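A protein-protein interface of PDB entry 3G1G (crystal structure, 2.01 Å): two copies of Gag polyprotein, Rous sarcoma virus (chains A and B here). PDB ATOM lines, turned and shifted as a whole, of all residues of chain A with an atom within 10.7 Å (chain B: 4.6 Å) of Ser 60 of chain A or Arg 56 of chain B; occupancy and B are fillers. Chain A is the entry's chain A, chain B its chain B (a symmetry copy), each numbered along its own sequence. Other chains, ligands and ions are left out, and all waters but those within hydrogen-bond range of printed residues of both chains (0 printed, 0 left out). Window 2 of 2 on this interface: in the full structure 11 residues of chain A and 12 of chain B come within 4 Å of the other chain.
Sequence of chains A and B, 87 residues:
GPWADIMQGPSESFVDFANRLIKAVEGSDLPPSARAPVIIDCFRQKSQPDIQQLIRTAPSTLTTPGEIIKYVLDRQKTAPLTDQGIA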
ATOM      1  N   PRO A  37     -18.065  -4.945  -4.148  1.00  0.00           N
ATOM      2  CA  PRO A  37     -16.753  -5.034  -4.838  1.00  0.00           C
ATOM      3  C   PRO A  37     -16.818  -4.821  -6.335  1.00  0.00           C
ATOM      4  O   PRO A  37     -15.970  -4.092  -6.917  1.00  0.00           O
ATOM      5  CB  PRO A  37     -16.314  -6.493  -4.565  1.00  0.00           C
ATOM      6  CG  PRO A  37     -17.013  -6.895  -3.343  1.00  0.00           C
ATOM      7  CD  PRO A  37     -18.182  -5.975  -3.095  1.00  0.00           C
ATOM      8  N   ILE A  40     -17.775  -1.055  -7.288  1.00  0.00           N
ATOM      9  CA  ILE A  40     -16.629  -0.158  -7.133  1.00  0.00           C
ATOM     10  C   ILE A  40     -15.589  -0.407  -8.234  1.00  0.00           C
ATOM     11  O   ILE A  40     -15.026   0.531  -8.801  1.00  0.00           O
ATOM     12  CB  ILE A  40     -16.056  -0.193  -5.669  1.00  0.00           C
ATOM     13  CG1 ILE A  40     -17.089   0.385  -4.702  1.00  0.00           C
ATOM     14  CG2 ILE A  40     -14.761   0.644  -5.527  1.00  0.00           C
ATOM     15  CD1 ILE A  40     -16.801  -0.059  -3.259  1.00  0.00           C
ATOM     16  N   ARG A  44     -14.180   2.298 -11.054  1.00  0.00           N
ATOM     17  CA  ARG A  44     -12.774   2.524 -11.387  1.00  0.00           C
ATOM     18  C   ARG A  44     -12.489   2.387 -12.874  1.00  0.00           C
ATOM     19  O   ARG A  44     -11.701   3.136 -13.432  1.00  0.00           O
ATOM     20  CB  ARG A  44     -11.880   1.572 -10.588  1.00  0.00           C
ATOM     21  CG  ARG A  44     -11.669   2.106  -9.188  1.00  0.00           C
ATOM     22  CD  ARG A  44     -10.532   1.370  -8.520  1.00  0.00           C
ATOM     23  NE  ARG A  44     -10.890  -0.016  -8.286  1.00  0.00           N
ATOM     24  CZ  ARG A  44     -11.236  -0.494  -7.095  1.00  0.00           C
ATOM     25  NH1 ARG A  44     -11.246   0.326  -6.037  1.00  0.00           N
ATOM     26  NH2 ARG A  44     -11.555  -1.786  -6.959  1.00  0.00           N
ATOM     27  N   LEU A  54     -10.032  10.833  -9.725  1.00  0.00           N
ATOM     28  CA  LEU A  54     -10.559  11.206  -8.443  1.00  0.00           C
ATOM     29  C   LEU A  54     -10.596   9.957  -7.560  1.00  0.00           C
ATOM     30  O   LEU A  54     -10.056   9.942  -6.456  1.00  0.00           O
ATOM     31  CB  LEU A  54     -11.960  11.761  -8.654  1.00  0.00           C
ATOM     32  CG  LEU A  54     -12.393  12.923  -7.808  1.00  0.00           C
ATOM     33  CD1 LEU A  54     -13.668  13.503  -8.383  1.00  0.00           C
ATOM     34  CD2 LEU A  54     -12.648  12.358  -6.434  1.00  0.00           C
ATOM     35  N   ILE A  55     -11.196   8.893  -8.081  1.00  0.00           N
ATOM     36  CA  ILE A  55     -11.281   7.635  -7.370  1.00  0.00           C
ATOM     37  C   ILE A  55      -9.889   6.999  -7.068  1.00  0.00           C
ATOM     38  O   ILE A  55      -9.702   6.434  -5.980  1.00  0.00           O
ATOM     39  CB  ILE A  55     -12.258   6.654  -8.096  1.00  0.00           C
ATOM     40  CG1 ILE A  55     -13.670   7.278  -8.191  1.00  0.00           C
ATOM     41  CG2 ILE A  55     -12.297   5.332  -7.424  1.00  0.00           C
ATOM     42  CD1 ILE A  55     -14.643   6.470  -8.997  1.00  0.00           C
ATOM     43  N   ARG A  56      -8.924   7.120  -7.982  1.00  0.00           N
ATOM     44  CA  ARG A  56      -7.552   6.592  -7.760  1.00  0.00           C
ATOM     45  C   ARG A  56      -6.966   7.010  -6.406  1.00  0.00           C
ATOM     46  O   ARG A  56      -6.216   6.256  -5.801  1.00  0.00           O
ATOM     47  CB  ARG A  56      -6.577   7.024  -8.876  1.00  0.00           C
ATOM     48  CG  ARG A  56      -6.096   5.923  -9.841  1.00  0.00           C
ATOM     49  CD  ARG A  56      -5.553   6.470 -11.216  1.00  0.00           C
ATOM     50  NE  ARG A  56      -6.134   5.714 -12.350  1.00  0.00           N
ATOM     51  CZ  ARG A  56      -6.707   6.239 -13.448  1.00  0.00           C
ATOM     52  NH1 ARG A  56      -6.748   7.560 -13.655  1.00  0.00           N
ATOM     53  NH2 ARG A  56      -7.218   5.429 -14.382  1.00  0.00           N
ATOM     54  N   THR A  57      -7.316   8.204  -5.941  1.00  0.00           N
ATOM     55  CA  THR A  57      -6.749   8.754  -4.720  1.00  0.00           C
ATOM     56  C   THR A  57      -7.661   8.640  -3.490  1.00  0.00           C
ATOM     57  O   THR A  57      -7.293   9.076  -2.407  1.00  0.00           O
ATOM     58  CB  THR A  57      -6.266  10.221  -4.927  1.00  0.00           C
ATOM     59  OG1 THR A  57      -7.359  11.044  -5.388  1.00  0.00           O
ATOM     60  CG2 THR A  57      -5.104  10.263  -5.945  1.00  0.00           C
ATOM     61  N   ALA A  58      -8.839   8.047  -3.651  1.00  0.00           N
ATOM     62  CA  ALA A  58      -9.727   7.794  -2.515  1.00  0.00           C
ATOM     63  C   ALA A  58      -9.163   6.760  -1.508  1.00  0.00           C
ATOM     64  O   ALA A  58      -8.582   5.746  -1.902  1.00  0.00           O
ATOM     65  CB  ALA A  58     -11.107   7.357  -3.006  1.00  0.00           C
ATOM     66  N   PRO A  59      -9.342   7.015  -0.206  1.00  0.00           N
ATOM     67  CA  PRO A  59      -8.996   6.027   0.812  1.00  0.00           C
ATOM     68  C   PRO A  59      -9.627   4.632   0.585  1.00  0.00           C
ATOM     69  O   PRO A  59     -10.815   4.518   0.223  1.00  0.00           O
ATOM     70  CB  PRO A  59      -9.531   6.663   2.106  1.00  0.00           C
ATOM     71  CG  PRO A  59      -9.982   8.065   1.752  1.00  0.00           C
ATOM     72  CD  PRO A  59      -9.503   8.359   0.373  1.00  0.00           C
ATOM     73  N   SER A  60      -8.848   3.575   0.815  1.00  0.00           N
ATOM     74  CA  SER A  60      -9.365   2.213   0.630  1.00  0.00           C
ATOM     75  C   SER A  60     -10.273   1.733   1.782  1.00  0.00           C
ATOM     76  O   SER A  60     -10.803   0.611   1.746  1.00  0.00           O
ATOM     77  CB  SER A  60      -8.244   1.222   0.356  1.00  0.00           C
ATOM     78  OG  SER A  60      -7.651   0.861   1.574  1.00  0.00           O
ATOM     79  N   THR A  61     -10.466   2.604   2.777  1.00  0.00           N
ATOM     80  CA  THR A  61     -11.506   2.448   3.799  1.00  0.00           C
ATOM     81  C   THR A  61     -12.916   2.775   3.256  1.00  0.00           C
ATOM     82  O   THR A  61     -13.925   2.467   3.903  1.00  0.00           O
ATOM     83  CB  THR A  61     -11.216   3.374   5.004  1.00  0.00           C
ATOM     84  OG1 THR A  61     -10.819   4.658   4.513  1.00  0.00           O
ATOM     85  CG2 THR A  61     -10.086   2.790   5.888  1.00  0.00           C
ATOM     86  N   LEU A  62     -12.987   3.412   2.080  1.00  0.00           N
ATOM     87  CA  LEU A  62     -14.279   3.726   1.472  1.00  0.00           C
ATOM     88  C   LEU A  62     -14.714   2.567   0.597  1.00  0.00           C
ATOM     89  O   LEU A  62     -14.391   2.520  -0.593  1.00  0.00           O
ATOM     90  CB  LEU A  62     -14.193   4.992   0.631  1.00  0.00           C
ATOM     91  CG  LEU A  62     -13.724   6.283   1.293  1.00  0.00           C
ATOM     92  CD1 LEU A  62     -13.956   7.456   0.349  1.00  0.00           C
ATOM     93  CD2 LEU A  62     -14.463   6.473   2.626  1.00  0.00           C
ATOM     94  N   THR A  63     -15.464   1.637   1.170  1.00  0.00           N
ATOM     95  CA  THR A  63     -15.648   0.363   0.494  1.00  0.00           C
ATOM     96  C   THR A  63     -17.091   0.077   0.128  1.00  0.00           C
ATOM     97  O   THR A  63     -17.396  -1.014  -0.339  1.00  0.00           O
ATOM     98  CB  THR A  63     -15.085  -0.809   1.332  1.00  0.00           C
ATOM     99  OG1 THR A  63     -15.676  -0.790   2.642  1.00  0.00           O
ATOM    100  CG2 THR A  63     -13.580  -0.710   1.458  1.00  0.00           C
ATOM    101  N   THR A  64     -17.983   1.035   0.379  1.00  0.00           N
ATOM    102  CA  THR A  64     -19.344   0.944  -0.123  1.00  0.00           C
ATOM    103  C   THR A  64     -19.461   1.885  -1.351  1.00  0.00           C
ATOM    104  O   THR A  64     -18.800   2.922  -1.408  1.00  0.00           O
ATOM    105  CB  THR A  64     -20.413   1.379   0.927  1.00  0.00           C
ATOM    106  OG1 THR A  64     -20.154   2.733   1.316  1.00  0.00           O
ATOM    107  CG2 THR A  64     -20.411   0.465   2.157  1.00  0.00           C
ATOM    108  N   PRO A  65     -20.290   1.511  -2.322  1.00  0.00           N
ATOM    109  CA  PRO A  65     -20.578   2.368  -3.476  1.00  0.00           C
ATOM    110  C   PRO A  65     -21.038   3.768  -3.023  1.00  0.00           C
ATOM    111  O   PRO A  65     -20.610   4.779  -3.591  1.00  0.00           O
ATOM    112  CB  PRO A  65     -21.728   1.619  -4.151  1.00  0.00           C
ATOM    113  CG  PRO A  65     -21.443   0.197  -3.839  1.00  0.00           C
ATOM    114  CD  PRO A  65     -21.019   0.230  -2.410  1.00  0.00           C
ATOM    115  N   GLU A  67     -20.302   5.508  -0.279  1.00  0.00           N
ATOM    116  CA  GLU A  67     -19.159   6.333   0.174  1.00  0.00           C
ATOM    117  C   GLU A  67     -18.346   6.882  -0.973  1.00  0.00           C
ATOM    118  O   GLU A  67     -17.896   8.019  -0.947  1.00  0.00           O
ATOM    119  CB  GLU A  67     -18.235   5.488   1.050  1.00  0.00           C
ATOM    120  CG  GLU A  67     -18.803   5.266   2.446  1.00  0.00           C
ATOM    121  CD  GLU A  67     -18.048   4.169   3.203  1.00  0.00           C
ATOM    122  OE1 GLU A  67     -17.947   3.031   2.691  1.00  0.00           O
ATOM    123  OE2 GLU A  67     -17.573   4.472   4.311  1.00  0.00           O
ATOM    124  N   ILE A  68     -18.121   6.052  -1.981  1.00  0.00           N
ATOM    125  CA  ILE A  68     -17.425   6.502  -3.172  1.00  0.00           C
ATOM    126  C   ILE A  68     -18.248   7.589  -3.850  1.00  0.00           C
ATOM    127  O   ILE A  68     -17.696   8.608  -4.231  1.00  0.00           O
ATOM    128  CB  ILE A  68     -17.164   5.375  -4.183  1.00  0.00           C
ATOM    129  CG1 ILE A  68     -16.323   4.288  -3.561  1.00  0.00           C
ATOM    130  CG2 ILE A  68     -16.310   5.913  -5.357  1.00  0.00           C
ATOM    131  CD1 ILE A  68     -14.884   4.716  -3.411  1.00  0.00           C
ATOM    132  N   TYR A  71     -17.804  10.790  -1.840  1.00  0.00           N
ATOM    133  CA  TYR A  71     -16.439  11.251  -2.064  1.00  0.00           C
ATOM    134  C   TYR A  71     -16.287  11.984  -3.410  1.00  0.00           C
ATOM    135  O   TYR A  71     -15.606  13.011  -3.481  1.00  0.00           O
ATOM    136  CB  TYR A  71     -15.458  10.057  -2.024  1.00  0.00           C
ATOM    137  CG  TYR A  71     -14.012  10.442  -2.180  1.00  0.00           C
ATOM    138  CD1 TYR A  71     -13.262  10.874  -1.088  1.00  0.00           C
ATOM    139  CD2 TYR A  71     -13.384  10.394  -3.427  1.00  0.00           C
ATOM    140  CE1 TYR A  71     -11.898  11.248  -1.235  1.00  0.00           C
ATOM    141  CE2 TYR A  71     -12.030  10.754  -3.583  1.00  0.00           C
ATOM    142  CZ  TYR A  71     -11.306  11.182  -2.494  1.00  0.00           C
ATOM    143  OH  TYR A  71      -9.980  11.528  -2.654  1.00  0.00           O
ATOM    144  N   ARG B  44      -9.622  -8.385   2.422  1.00  0.00           N
ATOM    145  CA  ARG B  44      -9.883  -7.286   3.339  1.00  0.00           C
ATOM    146  C   ARG B  44     -10.682  -7.721   4.537  1.00  0.00           C
ATOM    147  O   ARG B  44     -10.426  -7.235   5.625  1.00  0.00           O
ATOM    148  CB  ARG B  44     -10.620  -6.134   2.641  1.00  0.00           C
ATOM    149  CG  ARG B  44      -9.776  -5.411   1.608  1.00  0.00           C
ATOM    150  CD  ARG B  44     -10.434  -4.068   1.260  1.00  0.00           C
ATOM    151  NE  ARG B  44     -10.007  -3.648  -0.083  1.00  0.00           N
ATOM    152  CZ  ARG B  44      -8.983  -2.824  -0.329  1.00  0.00           C
ATOM    153  NH1 ARG B  44      -8.280  -2.308   0.683  1.00  0.00           N
ATOM    154  NH2 ARG B  44      -8.666  -2.493  -1.585  1.00  0.00           N
ATOM    155  N   GLN B  52      -5.613  -7.701   8.024  1.00  0.00           N
ATOM    156  CA  GLN B  52      -6.707  -6.774   7.676  1.00  0.00           C
ATOM    157  C   GLN B  52      -6.245  -5.329   7.852  1.00  0.00           C
ATOM    158  O   GLN B  52      -6.472  -4.466   6.988  1.00  0.00           O
ATOM    159  CB  GLN B  52      -7.922  -7.069   8.530  1.00  0.00           C
ATOM    160  CG  GLN B  52      -8.653  -8.343   8.086  1.00  0.00           C
ATOM    161  CD  GLN B  52      -9.964  -8.596   8.821  1.00  0.00           C
ATOM    162  OE1 GLN B  52     -10.655  -7.664   9.213  1.00  0.00           O
ATOM    163  NE2 GLN B  52     -10.343  -9.881   8.951  1.00  0.00           N
ATOM    164  N   GLN B  53      -5.562  -5.088   8.961  1.00  0.00           N
ATOM    165  CA  GLN B  53      -5.050  -3.765   9.299  1.00  0.00           C
ATOM    166  C   GLN B  53      -3.943  -3.357   8.344  1.00  0.00           C
ATOM    167  O   GLN B  53      -3.941  -2.242   7.838  1.00  0.00           O
ATOM    168  CB  GLN B  53      -4.523  -3.748  10.735  1.00  0.00           C
ATOM    169  CG  GLN B  53      -4.401  -2.328  11.303  1.00  0.00           C
ATOM    170  CD  GLN B  53      -5.702  -1.513  11.139  1.00  0.00           C
ATOM    171  OE1 GLN B  53      -6.764  -1.920  11.606  1.00  0.00           O
ATOM    172  NE2 GLN B  53      -5.618  -0.376  10.435  1.00  0.00           N
ATOM    173  N   LEU B  54      -2.996  -4.266   8.123  1.00  0.00           N
ATOM    174  CA  LEU B  54      -1.948  -4.088   7.093  1.00  0.00           C
ATOM    175  C   LEU B  54      -2.577  -3.705   5.750  1.00  0.00           C
ATOM    176  O   LEU B  54      -2.208  -2.698   5.160  1.00  0.00           O
ATOM    177  CB  LEU B  54      -1.101  -5.363   6.971  1.00  0.00           C
ATOM    178  CG  LEU B  54       0.356  -5.368   6.537  1.00  0.00           C
ATOM    179  CD1 LEU B  54       1.026  -6.543   7.211  1.00  0.00           C
ATOM    180  CD2 LEU B  54       0.487  -5.512   5.047  1.00  0.00           C
ATOM    181  N   ILE B  55      -3.585  -4.465   5.319  1.00  0.00           N
ATOM    182  CA  ILE B  55      -4.284  -4.176   4.069  1.00  0.00           C
ATOM    183  C   ILE B  55      -4.951  -2.784   4.067  1.00  0.00           C
ATOM    184  O   ILE B  55      -4.867  -2.091   3.074  1.00  0.00           O
ATOM    185  CB  ILE B  55      -5.240  -5.351   3.627  1.00  0.00           C
ATOM    186  CG1 ILE B  55      -4.391  -6.545   3.135  1.00  0.00           C
ATOM    187  CG2 ILE B  55      -6.198  -4.909   2.540  1.00  0.00           C
ATOM    188  CD1 ILE B  55      -5.111  -7.901   3.016  1.00  0.00           C
ATOM    189  N   ARG B  56      -5.537  -2.364   5.195  1.00  0.00           N
ATOM    190  CA  ARG B  56      -6.208  -1.059   5.318  1.00  0.00           C
ATOM    191  C   ARG B  56      -5.273   0.097   4.928  1.00  0.00           C
ATOM    192  O   ARG B  56      -5.708   1.070   4.331  1.00  0.00           O
ATOM    193  CB  ARG B  56      -6.762  -0.846   6.749  1.00  0.00           C
ATOM    194  CG  ARG B  56      -8.204  -1.346   7.001  1.00  0.00           C
ATOM    195  CD  ARG B  56      -8.625  -1.318   8.517  1.00  0.00           C
ATOM    196  NE  ARG B  56      -9.565  -2.422   8.778  1.00  0.00           N
ATOM    197  CZ  ARG B  56      -9.502  -3.352   9.751  1.00  0.00           C
ATOM    198  NH1 ARG B  56      -8.557  -3.349  10.721  1.00  0.00           N
ATOM    199  NH2 ARG B  56     -10.448  -4.311   9.761  1.00  0.00           N
ATOM    200  N   THR B  57      -3.989  -0.037   5.249  1.00  0.00           N
ATOM    201  CA  THR B  57      -2.966   0.979   4.947  1.00  0.00           C
ATOM    202  C   THR B  57      -2.396   0.947   3.507  1.00  0.00           C
ATOM    203  O   THR B  57      -1.448   1.665   3.217  1.00  0.00           O
ATOM    204  CB  THR B  57      -1.728   0.769   5.834  1.00  0.00           C
ATOM    205  OG1 THR B  57      -0.956  -0.327   5.297  1.00  0.00           O
ATOM    206  CG2 THR B  57      -2.116   0.510   7.313  1.00  0.00           C
ATOM    207  N   ALA B  58      -2.913   0.093   2.626  1.00  0.00           N
ATOM    208  CA  ALA B  58      -2.281  -0.092   1.311  1.00  0.00           C
ATOM    209  C   ALA B  58      -2.848   0.854   0.259  1.00  0.00           C
ATOM    210  O   ALA B  58      -4.079   1.042   0.187  1.00  0.00           O
ATOM    211  CB  ALA B  58      -2.404  -1.530   0.843  1.00  0.00           C
ATOM    212  N   SER B  60      -4.607   2.551  -2.705  1.00  0.00           N
ATOM    213  CA  SER B  60      -5.752   2.024  -3.466  1.00  0.00           C
ATOM    214  C   SER B  60      -5.461   1.894  -4.974  1.00  0.00           C
ATOM    215  O   SER B  60      -6.343   1.536  -5.759  1.00  0.00           O
ATOM    216  CB  SER B  60      -7.062   2.783  -3.185  1.00  0.00           C
ATOM    217  OG  SER B  60      -6.958   4.153  -3.513  1.00  0.00           O
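The side-chain amide oxygen (OE1) of Gln 53 of chain B is in hydrogen-bond range of the guanidinium group (NH1) of Arg 56 of chain B. The guanidinium group (NH2) of Arg 56 of chain B sits at hydrogen-bond distance from the side-chain amide oxygen (OE1) of Gln 52 of chain B (3.4 Å).
Arg 56 of chain A touches Ser 60 of chain B, and with the chains exchanged Ser 60 of chain A touches Arg 56 of chain B. Ala 58 of chain A touches Ser 60 of chain B, and with the chains exchanged Ser 60 of chain A touches Ala 58 of chain B. Ser 60 of chain A touches Arg 44 of chain B, but with the chains exchanged Arg 44 of chain A does not touch Ser 60 of chain B (5.0 Å). 7 positions are printed for both chains. Of the 5 pairs that touch across the chains among the printed residues, 4 have their exchanged pair printed and touching as well.
OG of Ser 60 of chain B is in hydrogen-bond range of O of Arg 56 of chain A, 3.2 Å away. O of Ala 58 of chain A is in hydrogen-bond range of OG of Ser 60 of chain B, at 2.8 Å. O of Arg 56 of chain B lies within hydrogen-bond range of OG of Ser 60 of chain A, at 3.4 Å. The side-chain hydroxyl (OG) of Ser 60 of chain A is in hydrogen-bond range of the guanidinium group (NH1) of Arg 44 of chain B (3.4 Å).
Ser 60 of chain A touches Ala 58 of chain B (OG to O, 3.8 Å).
Of chain B, only Arg 44, Arg 56 and Ala 58 come within 4 Å of Ser 60 of chain A. Of the printed residues of chain A, Arg 56 of chain B touches Ser 60. No residue of chain A comes within 4 Å of Thr 57 of chain B. Of the printed residues of chain B, Ala 58 of chain A touches Ser 60. Of the printed residues of chain B, Arg 56 of chain A touches Ser 60. Of the printed residues of chain A, Arg 44 of chain B touches Ser 60. Thr 63 of chain A touches none of the printed residues of chain B. Ile 40 of chain A touches none of the printed residues of chain B. The nearest residue of chain A that does not touch Arg 56 of chain B is Thr 61 of chain A (4.7 Å).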
